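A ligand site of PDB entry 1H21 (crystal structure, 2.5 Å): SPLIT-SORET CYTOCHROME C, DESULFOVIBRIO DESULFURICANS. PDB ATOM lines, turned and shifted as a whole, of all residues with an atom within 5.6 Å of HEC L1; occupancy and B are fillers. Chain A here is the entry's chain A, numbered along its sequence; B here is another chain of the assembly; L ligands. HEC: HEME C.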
ATOM      1  N   SER A 205       2.254 -22.962 -15.240  1.00  0.00           N
ATOM      2  CA  SER A 205       1.075 -23.821 -15.321  1.00  0.00           C
ATOM      3  C   SER A 205      -0.214 -23.001 -15.386  1.00  0.00           C
ATOM      4  O   SER A 205      -1.078 -23.271 -16.226  1.00  0.00           O
ATOM      5  CB  SER A 205       1.047 -24.785 -14.143  1.00  0.00           C
ATOM      6  OG  SER A 205       0.895 -24.087 -12.939  1.00  0.00           O
ATOM      7  N   SER A 208      -0.605 -21.581 -18.961  1.00  0.00           N
ATOM      8  CA  SER A 208      -0.920 -22.579 -20.000  1.00  0.00           C
ATOM      9  C   SER A 208      -2.236 -23.317 -19.800  1.00  0.00           C
ATOM     10  O   SER A 208      -3.014 -23.477 -20.726  1.00  0.00           O
ATOM     11  CB  SER A 208       0.250 -23.563 -20.225  1.00  0.00           C
ATOM     12  OG  SER A 208       0.576 -24.295 -19.067  1.00  0.00           O
ATOM     13  N   CYS A 209      -2.477 -23.780 -18.585  1.00  0.00           N
ATOM     14  CA  CYS A 209      -3.738 -24.474 -18.295  1.00  0.00           C
ATOM     15  C   CYS A 209      -4.838 -23.427 -18.439  1.00  0.00           C
ATOM     16  O   CYS A 209      -5.900 -23.723 -19.014  1.00  0.00           O
ATOM     17  CB  CYS A 209      -3.735 -25.006 -16.859  1.00  0.00           C
ATOM     18  SG  CYS A 209      -2.366 -26.117 -16.435  1.00  0.00           S
ATOM     19  N   GLU A 211      -5.287 -21.217 -20.443  1.00  0.00           N
ATOM     20  CA  GLU A 211      -5.698 -21.002 -21.841  1.00  0.00           C
ATOM     21  C   GLU A 211      -7.080 -21.581 -22.108  1.00  0.00           C
ATOM     22  O   GLU A 211      -7.878 -21.019 -22.877  1.00  0.00           O
ATOM     23  CB  GLU A 211      -4.678 -21.618 -22.803  1.00  0.00           C
ATOM     24  CG  GLU A 211      -3.292 -20.997 -22.666  1.00  0.00           C
ATOM     25  CD  GLU A 211      -2.948 -19.992 -23.768  1.00  0.00           C
ATOM     26  OE1 GLU A 211      -1.787 -19.529 -23.782  1.00  0.00           O
ATOM     27  OE2 GLU A 211      -3.823 -19.666 -24.610  1.00  0.00           O
ATOM     28  N   CYS A 212      -7.352 -22.726 -21.487  1.00  0.00           N
ATOM     29  CA  CYS A 212      -8.661 -23.371 -21.641  1.00  0.00           C
ATOM     30  C   CYS A 212      -9.546 -23.211 -20.405  1.00  0.00           C
ATOM     31  O   CYS A 212     -10.701 -22.832 -20.513  1.00  0.00           O
ATOM     32  CB  CYS A 212      -8.492 -24.868 -21.921  1.00  0.00           C
ATOM     33  SG  CYS A 212      -7.486 -25.260 -23.351  1.00  0.00           S
ATOM     34  N   HIS A 213      -8.959 -23.447 -19.245  1.00  0.00           N
ATOM     35  CA  HIS A 213      -9.689 -23.418 -17.999  1.00  0.00           C
ATOM     36  C   HIS A 213      -9.987 -22.078 -17.364  1.00  0.00           C
ATOM     37  O   HIS A 213     -10.858 -22.007 -16.494  1.00  0.00           O
ATOM     38  CB  HIS A 213      -9.059 -24.384 -17.016  1.00  0.00           C
ATOM     39  CG  HIS A 213      -9.095 -25.799 -17.495  1.00  0.00           C
ATOM     40  ND1 HIS A 213     -10.258 -26.525 -17.657  1.00  0.00           N
ATOM     41  CD2 HIS A 213      -8.091 -26.619 -17.912  1.00  0.00           C
ATOM     42  CE1 HIS A 213      -9.946 -27.728 -18.148  1.00  0.00           C
ATOM     43  NE2 HIS A 213      -8.644 -27.843 -18.323  1.00  0.00           N
ATOM     44  N   ASN A 218     -14.278 -20.117 -23.625  1.00  0.00           N
ATOM     45  CA  ASN A 218     -13.776 -21.480 -23.835  1.00  0.00           C
ATOM     46  C   ASN A 218     -14.735 -22.518 -23.306  1.00  0.00           C
ATOM     47  O   ASN A 218     -15.316 -22.381 -22.219  1.00  0.00           O
ATOM     48  CB  ASN A 218     -12.394 -21.689 -23.202  1.00  0.00           C
ATOM     49  CG  ASN A 218     -11.634 -22.864 -23.829  1.00  0.00           C
ATOM     50  OD1 ASN A 218     -12.042 -24.024 -23.714  1.00  0.00           O
ATOM     51  ND2 ASN A 218     -10.524 -22.555 -24.502  1.00  0.00           N
ATOM     52  N   ASP A 219     -14.838 -23.610 -24.056  1.00  0.00           N
ATOM     53  CA  ASP A 219     -15.714 -24.718 -23.706  1.00  0.00           C
ATOM     54  C   ASP A 219     -15.271 -25.428 -22.429  1.00  0.00           C
ATOM     55  O   ASP A 219     -16.051 -26.190 -21.848  1.00  0.00           O
ATOM     56  CB  ASP A 219     -15.779 -25.693 -24.877  1.00  0.00           C
ATOM     57  CG  ASP A 219     -16.111 -24.999 -26.212  1.00  0.00           C
ATOM     58  OD1 ASP A 219     -17.106 -25.400 -26.852  1.00  0.00           O
ATOM     59  OD2 ASP A 219     -15.371 -24.074 -26.638  1.00  0.00           O
ATOM     60  N   ALA A 220     -14.054 -25.151 -22.000  1.00  0.00           N
ATOM     61  CA  ALA A 220     -13.486 -25.770 -20.803  1.00  0.00           C
ATOM     62  C   ALA A 220     -13.268 -24.767 -19.660  1.00  0.00           C
ATOM     63  O   ALA A 220     -12.683 -25.102 -18.627  1.00  0.00           O
ATOM     64  CB  ALA A 220     -12.183 -26.439 -21.167  1.00  0.00           C
ATOM     65  N   TRP A 222     -13.936 -23.626 -16.731  1.00  0.00           N
ATOM     66  CA  TRP A 222     -14.588 -23.961 -15.462  1.00  0.00           C
ATOM     67  C   TRP A 222     -13.852 -23.553 -14.190  1.00  0.00           C
ATOM     68  O   TRP A 222     -14.481 -23.345 -13.158  1.00  0.00           O
ATOM     69  CB  TRP A 222     -14.792 -25.474 -15.370  1.00  0.00           C
ATOM     70  CG  TRP A 222     -15.481 -26.071 -16.517  1.00  0.00           C
ATOM     71  CD1 TRP A 222     -16.711 -25.736 -16.997  1.00  0.00           C
ATOM     72  CD2 TRP A 222     -14.977 -27.116 -17.349  1.00  0.00           C
ATOM     73  NE1 TRP A 222     -17.006 -26.517 -18.088  1.00  0.00           N
ATOM     74  CE2 TRP A 222     -15.969 -27.367 -18.330  1.00  0.00           C
ATOM     75  CE3 TRP A 222     -13.794 -27.866 -17.366  1.00  0.00           C
ATOM     76  CZ2 TRP A 222     -15.807 -28.333 -19.320  1.00  0.00           C
ATOM     77  CZ3 TRP A 222     -13.628 -28.823 -18.356  1.00  0.00           C
ATOM     78  CH2 TRP A 222     -14.637 -29.045 -19.324  1.00  0.00           C
ATOM     79  N   CYS A 229      -0.903 -24.829 -10.390  1.00  0.00           N
ATOM     80  CA  CYS A 229      -1.603 -26.101 -10.587  1.00  0.00           C
ATOM     81  C   CYS A 229      -0.782 -27.373 -10.391  1.00  0.00           C
ATOM     82  O   CYS A 229      -1.348 -28.425 -10.120  1.00  0.00           O
ATOM     83  CB  CYS A 229      -2.196 -26.110 -11.983  1.00  0.00           C
ATOM     84  SG  CYS A 229      -2.765 -24.500 -12.487  1.00  0.00           S
ATOM     85  N   HIS A 233      -2.337 -31.340  -9.760  1.00  0.00           N
ATOM     86  CA  HIS A 233      -2.701 -31.894 -11.047  1.00  0.00           C
ATOM     87  C   HIS A 233      -1.558 -32.550 -11.830  1.00  0.00           C
ATOM     88  O   HIS A 233      -1.568 -32.578 -13.060  1.00  0.00           O
ATOM     89  CB  HIS A 233      -3.437 -30.802 -11.853  1.00  0.00           C
ATOM     90  CG  HIS A 233      -4.747 -30.374 -11.232  1.00  0.00           C
ATOM     91  ND1 HIS A 233      -5.831 -31.210 -11.069  1.00  0.00           N
ATOM     92  CD2 HIS A 233      -5.170 -29.154 -10.833  1.00  0.00           C
ATOM     93  CE1 HIS A 233      -6.864 -30.503 -10.595  1.00  0.00           C
ATOM     94  NE2 HIS A 233      -6.527 -29.232 -10.429  1.00  0.00           N
ATOM     95  N   TYR B 156     -17.760 -27.602 -13.749  1.00  0.00           N
ATOM     96  CA  TYR B 156     -17.450 -28.754 -14.569  1.00  0.00           C
ATOM     97  C   TYR B 156     -18.644 -29.714 -14.689  1.00  0.00           C
ATOM     98  O   TYR B 156     -19.109 -29.999 -15.801  1.00  0.00           O
ATOM     99  CB  TYR B 156     -16.254 -29.485 -13.955  1.00  0.00           C
ATOM    100  CG  TYR B 156     -15.886 -30.801 -14.616  1.00  0.00           C
ATOM    101  CD1 TYR B 156     -15.520 -30.857 -15.953  1.00  0.00           C
ATOM    102  CD2 TYR B 156     -15.919 -31.982 -13.881  1.00  0.00           C
ATOM    103  CE1 TYR B 156     -15.200 -32.065 -16.565  1.00  0.00           C
ATOM    104  CE2 TYR B 156     -15.589 -33.207 -14.478  1.00  0.00           C
ATOM    105  CZ  TYR B 156     -15.236 -33.234 -15.825  1.00  0.00           C
ATOM    106  OH  TYR B 156     -14.945 -34.450 -16.441  1.00  0.00           O
ATOM    107  N   ALA B 237      -9.424 -39.080 -11.539  1.00  0.00           N
ATOM    108  CA  ALA B 237      -9.019 -38.642 -12.871  1.00  0.00           C
ATOM    109  C   ALA B 237      -8.440 -37.215 -12.774  1.00  0.00           C
ATOM    110  O   ALA B 237      -7.429 -36.894 -13.415  1.00  0.00           O
ATOM    111  CB  ALA B 237     -10.213 -38.645 -13.789  1.00  0.00           C
ATOM    112  N   ALA B 238      -9.053 -36.397 -11.928  1.00  0.00           N
ATOM    113  CA  ALA B 238      -8.635 -35.009 -11.750  1.00  0.00           C
ATOM    114  C   ALA B 238      -7.188 -34.825 -11.281  1.00  0.00           C
ATOM    115  O   ALA B 238      -6.480 -33.967 -11.798  1.00  0.00           O
ATOM    116  CB  ALA B 238      -9.594 -34.301 -10.796  1.00  0.00           C
ATOM    117  N   LYS B 242      -2.057 -33.895 -15.559  1.00  0.00           N
ATOM    118  CA  LYS B 242      -2.735 -33.112 -16.602  1.00  0.00           C
ATOM    119  C   LYS B 242      -1.728 -32.327 -17.457  1.00  0.00           C
ATOM    120  O   LYS B 242      -2.134 -31.587 -18.355  1.00  0.00           O
ATOM    121  CB  LYS B 242      -3.736 -32.145 -15.961  1.00  0.00           C
ATOM    122  CG  LYS B 242      -4.753 -32.829 -15.069  1.00  0.00           C
ATOM    123  CD  LYS B 242      -5.615 -33.759 -15.888  1.00  0.00           C
ATOM    124  CE  LYS B 242      -5.870 -35.066 -15.158  1.00  0.00           C
ATOM    125  NZ  LYS B 242      -6.577 -36.019 -16.061  1.00  0.00           N
ATOM    126  N   PHE B 243      -0.436 -32.477 -17.147  1.00  0.00           N
ATOM    127  CA  PHE B 243       0.650 -31.785 -17.876  1.00  0.00           C
ATOM    128  C   PHE B 243       1.157 -32.553 -19.105  1.00  0.00           C
ATOM    129  O   PHE B 243       1.825 -31.991 -19.975  1.00  0.00           O
ATOM    130  CB  PHE B 243       1.822 -31.495 -16.929  1.00  0.00           C
ATOM    131  CG  PHE B 243       1.536 -30.439 -15.882  1.00  0.00           C
ATOM    132  CD1 PHE B 243       0.988 -30.788 -14.658  1.00  0.00           C
ATOM    133  CD2 PHE B 243       1.828 -29.112 -16.127  1.00  0.00           C
ATOM    134  CE1 PHE B 243       0.734 -29.809 -13.679  1.00  0.00           C
ATOM    135  CE2 PHE B 243       1.582 -28.137 -15.153  1.00  0.00           C
ATOM    136  CZ  PHE B 243       1.043 -28.489 -13.932  1.00  0.00           C
ATOM    137  N   HIS B 246      -2.891 -34.363 -22.277  1.00  0.00           N
ATOM    138  CA  HIS B 246      -4.148 -33.815 -21.805  1.00  0.00           C
ATOM    139  C   HIS B 246      -4.450 -32.587 -22.612  1.00  0.00           C
ATOM    140  O   HIS B 246      -3.570 -31.749 -22.821  1.00  0.00           O
ATOM    141  CB  HIS B 246      -4.063 -33.466 -20.311  1.00  0.00           C
ATOM    142  CG  HIS B 246      -5.311 -32.815 -19.786  1.00  0.00           C
ATOM    143  ND1 HIS B 246      -6.451 -33.497 -19.412  1.00  0.00           N
ATOM    144  CD2 HIS B 246      -5.603 -31.495 -19.616  1.00  0.00           C
ATOM    145  CE1 HIS B 246      -7.361 -32.595 -19.058  1.00  0.00           C
ATOM    146  NE2 HIS B 246      -6.902 -31.360 -19.160  1.00  0.00           N
ATOM    147  N   PRO B 247      -5.676 -32.462 -23.140  1.00  0.00           N
ATOM    148  CA  PRO B 247      -6.761 -33.454 -22.980  1.00  0.00           C
ATOM    149  C   PRO B 247      -6.734 -34.657 -23.952  1.00  0.00           C
ATOM    150  O   PRO B 247      -5.647 -35.205 -24.236  1.00  0.00           O
ATOM    151  CB  PRO B 247      -8.029 -32.593 -23.127  1.00  0.00           C
ATOM    152  CG  PRO B 247      -7.608 -31.526 -24.077  1.00  0.00           C
ATOM    153  CD  PRO B 247      -6.198 -31.177 -23.625  1.00  0.00           C
ATOM    154  OXT PRO B 247      -7.816 -35.097 -24.415  1.00  0.00           O
HETATM  155 FE   HEC L   1      -7.868 -29.649 -18.692  1.00  0.00          FE
HETATM  156  CHA HEC L   1     -10.615 -31.580 -18.180  1.00  0.00           C
HETATM  157  CHB HEC L   1      -7.017 -29.864 -15.418  1.00  0.00           C
HETATM  158  CHC HEC L   1      -4.954 -27.987 -19.358  1.00  0.00           C
HETATM  159  CHD HEC L   1      -9.062 -28.879 -21.815  1.00  0.00           C
HETATM  160  NA  HEC L   1      -8.681 -30.487 -17.138  1.00  0.00           N
HETATM  161  C1A HEC L   1      -9.782 -31.316 -17.086  1.00  0.00           C
HETATM  162  C2A HEC L   1      -9.982 -31.833 -15.735  1.00  0.00           C
HETATM  163  C3A HEC L   1      -9.044 -31.286 -14.907  1.00  0.00           C
HETATM  164  C4A HEC L   1      -8.212 -30.468 -15.800  1.00  0.00           C
HETATM  165  CMA HEC L   1      -8.952 -31.455 -13.394  1.00  0.00           C
HETATM  166  CAA HEC L   1     -11.081 -32.803 -15.342  1.00  0.00           C
HETATM  167  CBA HEC L   1     -10.715 -34.230 -15.057  1.00  0.00           C
HETATM  168  CGA HEC L   1     -10.098 -34.956 -16.234  1.00  0.00           C
HETATM  169  O1A HEC L   1      -8.980 -34.638 -16.663  1.00  0.00           O
HETATM  170  O2A HEC L   1     -10.713 -35.934 -16.700  1.00  0.00           O
HETATM  171  NB  HEC L   1      -6.281 -29.077 -17.666  1.00  0.00           N
HETATM  172  C1B HEC L   1      -6.120 -29.213 -16.283  1.00  0.00           C
HETATM  173  C2B HEC L   1      -4.885 -28.581 -15.800  1.00  0.00           C
HETATM  174  C3B HEC L   1      -4.187 -28.158 -16.935  1.00  0.00           C
HETATM  175  C4B HEC L   1      -5.132 -28.418 -18.080  1.00  0.00           C
HETATM  176  CMB HEC L   1      -4.589 -28.311 -14.333  1.00  0.00           C
HETATM  177  CAB HEC L   1      -2.801 -27.765 -17.009  1.00  0.00           C
HETATM  178  CBB HEC L   1      -1.694 -28.518 -16.417  1.00  0.00           C
HETATM  179  NC  HEC L   1      -7.093 -28.756 -20.287  1.00  0.00           N
HETATM  180  C1C HEC L   1      -5.863 -28.129 -20.402  1.00  0.00           C
HETATM  181  C2C HEC L   1      -5.761 -27.363 -21.635  1.00  0.00           C
HETATM  182  C3C HEC L   1      -6.950 -27.567 -22.312  1.00  0.00           C
HETATM  183  C4C HEC L   1      -7.767 -28.442 -21.490  1.00  0.00           C
HETATM  184  CMC HEC L   1      -4.599 -26.403 -22.006  1.00  0.00           C
HETATM  185  CAC HEC L   1      -7.347 -27.030 -23.514  1.00  0.00           C
HETATM  186  CBC HEC L   1      -6.586 -27.267 -24.709  1.00  0.00           C
HETATM  187  ND  HEC L   1      -9.468 -30.178 -19.769  1.00  0.00           N
HETATM  188  C1D HEC L   1      -9.861 -29.716 -21.022  1.00  0.00           C
HETATM  189  C2D HEC L   1     -11.161 -30.291 -21.408  1.00  0.00           C
HETATM  190  C3D HEC L   1     -11.518 -31.112 -20.432  1.00  0.00           C
HETATM  191  C4D HEC L   1     -10.486 -31.027 -19.426  1.00  0.00           C
HETATM  192  CMD HEC L   1     -12.011 -29.956 -22.639  1.00  0.00           C
HETATM  193  CAD HEC L   1     -12.797 -31.928 -20.314  1.00  0.00           C
HETATM  194  CBD HEC L   1     -12.916 -33.070 -21.314  1.00  0.00           C
HETATM  195  CGD HEC L   1     -11.794 -34.072 -21.167  1.00  0.00           C
HETATM  196  O1D HEC L   1     -10.814 -33.981 -21.947  1.00  0.00           O
HETATM  197  O2D HEC L   1     -11.914 -34.955 -20.285  1.00  0.00           O
HETATM  198 FE   HEC L   2      -7.755 -27.782  -9.708  1.00  0.00          FE
HETATM  199  CHA HEC L   2     -10.778 -29.357  -9.855  1.00  0.00           C
HETATM  200  CHB HEC L   2      -7.979 -26.938 -12.940  1.00  0.00           C
HETATM  201  CHC HEC L   2      -5.202 -25.768  -9.271  1.00  0.00           C
HETATM  202  CHD HEC L   2      -7.067 -29.384  -6.763  1.00  0.00           C
HETATM  203  NA  HEC L   2      -9.119 -28.000 -11.073  1.00  0.00           N
HETATM  204  C1A HEC L   2     -10.369 -28.596 -10.956  1.00  0.00           C
HETATM  205  C2A HEC L   2     -11.129 -28.459 -12.205  1.00  0.00           C
HETATM  206  C3A HEC L   2     -10.310 -27.817 -13.048  1.00  0.00           C
HETATM  207  C4A HEC L   2      -9.075 -27.569 -12.365  1.00  0.00           C
HETATM  208  CMA HEC L   2     -10.633 -27.483 -14.510  1.00  0.00           C
HETATM  209  CAA HEC L   2     -12.513 -29.025 -12.607  1.00  0.00           C
HETATM  210  CBA HEC L   2     -12.623 -30.467 -13.124  1.00  0.00           C
HETATM  211  CGA HEC L   2     -12.667 -31.506 -12.022  1.00  0.00           C
HETATM  212  O1A HEC L   2     -11.889 -32.479 -12.098  1.00  0.00           O
HETATM  213  O2A HEC L   2     -13.487 -31.353 -11.085  1.00  0.00           O
HETATM  214  NB  HEC L   2      -6.799 -26.612 -10.867  1.00  0.00           N
HETATM  215  C1B HEC L   2      -6.910 -26.469 -12.221  1.00  0.00           C
HETATM  216  C2B HEC L   2      -6.015 -25.521 -12.751  1.00  0.00           C
HETATM  217  C3B HEC L   2      -5.308 -24.993 -11.689  1.00  0.00           C
HETATM  218  C4B HEC L   2      -5.818 -25.735 -10.511  1.00  0.00           C
HETATM  219  CMB HEC L   2      -5.987 -25.180 -14.218  1.00  0.00           C
HETATM  220  CAB HEC L   2      -4.302 -24.001 -11.665  1.00  0.00           C
HETATM  221  CBB HEC L   2      -4.558 -22.592 -11.710  1.00  0.00           C
HETATM  222  NC  HEC L   2      -6.442 -27.553  -8.305  1.00  0.00           N
HETATM  223  C1C HEC L   2      -5.433 -26.642  -8.269  1.00  0.00           C
HETATM  224  C2C HEC L   2      -4.641 -26.812  -7.079  1.00  0.00           C
HETATM  225  C3C HEC L   2      -5.179 -27.868  -6.380  1.00  0.00           C
HETATM  226  C4C HEC L   2      -6.278 -28.308  -7.148  1.00  0.00           C
HETATM  227  CMC HEC L   2      -3.416 -25.979  -6.677  1.00  0.00           C
HETATM  228  CAC HEC L   2      -4.788 -28.425  -5.170  1.00  0.00           C
HETATM  229  CBC HEC L   2      -4.866 -27.676  -3.923  1.00  0.00           C
HETATM  230  ND  HEC L   2      -8.690 -29.095  -8.566  1.00  0.00           N
HETATM  231  C1D HEC L   2      -8.200 -29.770  -7.444  1.00  0.00           C
HETATM  232  C2D HEC L   2      -9.145 -30.831  -6.999  1.00  0.00           C
HETATM  233  C3D HEC L   2     -10.249 -30.720  -7.790  1.00  0.00           C
HETATM  234  C4D HEC L   2      -9.974 -29.648  -8.760  1.00  0.00           C
HETATM  235  CMD HEC L   2      -8.926 -31.861  -5.920  1.00  0.00           C
HETATM  236  CAD HEC L   2     -11.561 -31.510  -7.667  1.00  0.00           C
HETATM  237  CBD HEC L   2     -11.682 -32.687  -8.633  1.00  0.00           C
HETATM  238  CGD HEC L   2     -13.009 -33.392  -8.497  1.00  0.00           C
HETATM  239  O1D HEC L   2     -13.956 -32.935  -9.139  1.00  0.00           O
HETATM  240  O2D HEC L   2     -13.131 -34.356  -7.707  1.00  0.00           O
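NE2 of His 246 of chain B is bound to FE of HEC L1 (2.0 Å). The side-chain sulfur (SG) of Cys 229 is covalently linked to a carbon (CAB) of HEC L2 (1.8 Å). FE of HEC L1 is bound by NE2 of His 213. The side-chain sulfur of Cys 209 is covalently linked to a carbon (CAB) of HEC L1 (1.8 Å). The side-chain amino group (NZ) of Lys 242 of chain B lies within salt-bridge range of an oxygen (O1A) of HEC L1. A ring nitrogen (NE2) of His 233 is bound to an iron atom (FE) of HEC L2, at 2.0 Å. CAC of HEC L1 is covalently linked to SG of Cys 212 (1.8 Å).
The backbone carbonyl oxygen (O) of Ala 237 of chain B sits at hydrogen-bond distance from the side-chain amino group (NZ) of Lys 242 of chain B (2.9 Å). OG of Ser 208 sits at hydrogen-bond distance from O of Ser 205, 3.4 Å away. N of Ala 220 lies within hydrogen-bond range of OD1 of Asn 218, at 2.9 Å. O of Ala 238 of chain B lies within hydrogen-bond range of ND1 of His 233 (2.9 Å). ND1 of His 213 lies within hydrogen-bond range of O of Ala 220 (3.0 Å). The backbone NH of Trp 222 sits at hydrogen-bond distance from the backbone carbonyl oxygen of His 213. N of Lys 242 of chain B is in hydrogen-bond range of O of His 233, at 2.9 Å.
Merely in contact with HEC L1: Pro 247 of chain B (3.3 Å), Phe 243 of chain B (3.5 Å), Trp 222 (3.6 Å), Ser 208 (3.6 Å), His 233 (3.6 Å), Ala 220 (3.8 Å) and Ala 238 of chain B (3.9 Å). Hydrophobic or aromatic side chains within 4 Å of HEC L1: His 213, Ala 220, Trp 222, His 233, Ala 238 of chain B, Phe 243 of chain B, His 246 of chain B and Pro 247 of chain B. 12 residues have an atom within 4 Å of HEC L1: Ser 208, Cys 209, Cys 212, His 213, Ala 220, Trp 222, His 233, Ala 238 of chain B, Lys 242 of chain B, Phe 243 of chain B, His 246 of chain B and Pro 247 of chain B. The nearest printed residue that does not touch HEC L1 is Ala 237 of chain B (4.01 Å).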
